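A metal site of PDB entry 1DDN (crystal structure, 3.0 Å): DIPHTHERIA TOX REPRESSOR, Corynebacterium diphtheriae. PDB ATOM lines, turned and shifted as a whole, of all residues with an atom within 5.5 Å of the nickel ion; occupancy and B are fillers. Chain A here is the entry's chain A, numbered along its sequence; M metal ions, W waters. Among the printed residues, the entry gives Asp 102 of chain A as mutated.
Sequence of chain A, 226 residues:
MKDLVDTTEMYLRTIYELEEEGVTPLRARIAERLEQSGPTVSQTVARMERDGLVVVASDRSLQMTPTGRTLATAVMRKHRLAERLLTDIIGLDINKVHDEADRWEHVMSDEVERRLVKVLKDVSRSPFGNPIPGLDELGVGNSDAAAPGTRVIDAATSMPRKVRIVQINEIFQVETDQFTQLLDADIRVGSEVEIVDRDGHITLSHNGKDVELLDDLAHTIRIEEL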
ATOM      1  N   LEU A   4      25.496  26.827 -12.933  1.00  0.00           N
ATOM      2  CA  LEU A   4      25.525  25.436 -12.557  1.00  0.00           C
ATOM      3  C   LEU A   4      26.946  24.956 -12.306  1.00  0.00           C
ATOM      4  O   LEU A   4      27.152  23.799 -11.999  1.00  0.00           O
ATOM      5  CB  LEU A   4      24.856  24.604 -13.662  1.00  0.00           C
ATOM      6  CG  LEU A   4      23.320  24.464 -13.708  1.00  0.00           C
ATOM      7  CD1 LEU A   4      22.664  25.625 -13.012  1.00  0.00           C
ATOM      8  CD2 LEU A   4      22.842  24.402 -15.162  1.00  0.00           C
ATOM      9  N   VAL A   5      27.920  25.841 -12.403  1.00  0.00           N
ATOM     10  CA  VAL A   5      29.329  25.488 -12.221  1.00  0.00           C
ATOM     11  C   VAL A   5      29.714  24.440 -13.243  1.00  0.00           C
ATOM     12  O   VAL A   5      30.793  24.510 -13.825  1.00  0.00           O
ATOM     13  CB  VAL A   5      29.596  24.937 -10.819  1.00  0.00           C
ATOM     14  CG1 VAL A   5      31.059  24.509 -10.706  1.00  0.00           C
ATOM     15  CG2 VAL A   5      29.274  25.990  -9.779  1.00  0.00           C
ATOM     16  N   MET A  10      25.071  18.627 -13.207  1.00  0.00           N
ATOM     17  CA  MET A  10      23.786  18.989 -12.635  1.00  0.00           C
ATOM     18  C   MET A  10      22.615  18.312 -13.394  1.00  0.00           C
ATOM     19  O   MET A  10      21.491  18.251 -12.900  1.00  0.00           O
ATOM     20  CB  MET A  10      23.612  20.508 -12.630  1.00  0.00           C
ATOM     21  CG  MET A  10      24.618  21.233 -11.748  1.00  0.00           C
ATOM     22  SD  MET A  10      24.349  21.059  -9.944  1.00  0.00           S
ATOM     23  CE  MET A  10      22.564  21.017  -9.926  1.00  0.00           C
ATOM     24  N   ARG A  13      23.124  14.630 -11.890  1.00  0.00           N
ATOM     25  CA  ARG A  13      22.638  14.588 -10.528  1.00  0.00           C
ATOM     26  C   ARG A  13      21.128  14.688 -10.494  1.00  0.00           C
ATOM     27  O   ARG A  13      20.484  13.886  -9.835  1.00  0.00           O
ATOM     28  CB  ARG A  13      23.209  15.725  -9.686  1.00  0.00           C
ATOM     29  CG  ARG A  13      22.759  15.623  -8.248  1.00  0.00           C
ATOM     30  CD  ARG A  13      23.264  16.760  -7.437  1.00  0.00           C
ATOM     31  NE  ARG A  13      22.241  17.786  -7.293  1.00  0.00           N
ATOM     32  CZ  ARG A  13      22.334  18.800  -6.450  1.00  0.00           C
ATOM     33  NH1 ARG A  13      23.410  18.925  -5.683  1.00  0.00           N
ATOM     34  NH2 ARG A  13      21.349  19.703  -6.367  1.00  0.00           N
ATOM     35  N   ALA A 101      27.022  23.632  -1.226  1.00  0.00           N
ATOM     36  CA  ALA A 101      27.432  22.305  -1.672  1.00  0.00           C
ATOM     37  C   ALA A 101      27.059  22.160  -3.140  1.00  0.00           C
ATOM     38  O   ALA A 101      27.722  21.441  -3.885  1.00  0.00           O
ATOM     39  CB  ALA A 101      26.756  21.238  -0.859  1.00  0.00           C
ATOM     40  N   ASP A 102      26.016  22.859  -3.556  1.00  0.00           N
ATOM     41  CA  ASP A 102      25.576  22.799  -4.947  1.00  0.00           C
ATOM     42  C   ASP A 102      26.702  23.254  -5.879  1.00  0.00           C
ATOM     43  O   ASP A 102      26.725  22.874  -7.041  1.00  0.00           O
ATOM     44  CB  ASP A 102      24.341  23.680  -5.151  1.00  0.00           C
ATOM     45  CG  ASP A 102      23.623  23.412  -6.469  1.00  0.00           C
ATOM     46  OD1 ASP A 102      24.187  22.694  -7.331  1.00  0.00           O
ATOM     47  OD2 ASP A 102      22.491  23.906  -6.635  1.00  0.00           O
ATOM     48  N   ARG A 103      27.634  24.042  -5.362  1.00  0.00           N
ATOM     49  CA  ARG A 103      28.765  24.535  -6.169  1.00  0.00           C
ATOM     50  C   ARG A 103      29.997  23.670  -5.950  1.00  0.00           C
ATOM     51  O   ARG A 103      30.700  23.312  -6.898  1.00  0.00           O
ATOM     52  CB  ARG A 103      29.097  25.976  -5.802  1.00  0.00           C
ATOM     53  CG  ARG A 103      28.021  26.948  -6.203  1.00  0.00           C
ATOM     54  CD  ARG A 103      28.554  28.346  -6.423  1.00  0.00           C
ATOM     55  NE  ARG A 103      28.075  29.220  -5.365  1.00  0.00           N
ATOM     56  CZ  ARG A 103      28.475  29.108  -4.100  1.00  0.00           C
ATOM     57  NH1 ARG A 103      29.342  28.167  -3.792  1.00  0.00           N
ATOM     58  NH2 ARG A 103      28.012  29.912  -3.155  1.00  0.00           N
ATOM     59  N   GLU A 105      30.222  20.524  -5.093  1.00  0.00           N
ATOM     60  CA  GLU A 105      30.128  19.179  -5.683  1.00  0.00           C
ATOM     61  C   GLU A 105      30.889  19.046  -7.006  1.00  0.00           C
ATOM     62  O   GLU A 105      31.316  17.953  -7.380  1.00  0.00           O
ATOM     63  CB  GLU A 105      28.657  18.804  -5.909  1.00  0.00           C
ATOM     64  CG  GLU A 105      27.800  19.947  -6.433  1.00  0.00           C
ATOM     65  CD  GLU A 105      26.353  19.548  -6.682  1.00  0.00           C
ATOM     66  OE1 GLU A 105      25.929  18.514  -6.121  1.00  0.00           O
ATOM     67  OE2 GLU A 105      25.650  20.270  -7.423  1.00  0.00           O
ATOM     68  N   HIS A 106      31.061  20.175  -7.694  1.00  0.00           N
ATOM     69  CA  HIS A 106      31.735  20.182  -8.982  1.00  0.00           C
ATOM     70  C   HIS A 106      33.210  20.528  -8.960  1.00  0.00           C
ATOM     71  O   HIS A 106      33.808  20.724 -10.008  1.00  0.00           O
ATOM     72  CB  HIS A 106      31.005  21.132  -9.927  1.00  0.00           C
ATOM     73  CG  HIS A 106      29.519  21.032  -9.819  1.00  0.00           C
ATOM     74  ND1 HIS A 106      28.819  19.918 -10.217  1.00  0.00           N
ATOM     75  CD2 HIS A 106      28.614  21.864  -9.250  1.00  0.00           C
ATOM     76  CE1 HIS A 106      27.541  20.067  -9.896  1.00  0.00           C
ATOM     77  NE2 HIS A 106      27.394  21.235  -9.298  1.00  0.00           N
HETATM   78 NI    NI M   1      25.720  21.986  -8.450  1.00  0.00          NI
HETATM   79  O   HOH W   1      25.892  23.730  -9.521  1.00  0.00           O
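OE1 of Glu 105 is in salt-bridge range of NH1 of Arg 13, at 2.6 Å.
Of the 9 residues printed, 4 come within 4 Å of the nickel ion. The nearest printed residue that does not touch the nickel ion is Arg 103 (4.2 Å).
The nickel ion is bound by the backbone carbonyl oxygen of Asp 102, the side-chain carboxylate of Glu 105, a ring nitrogen (NE2) of His 106, the side-chain carboxylate of Asp 102, water W1 and the side-chain sulfur of Met 10.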
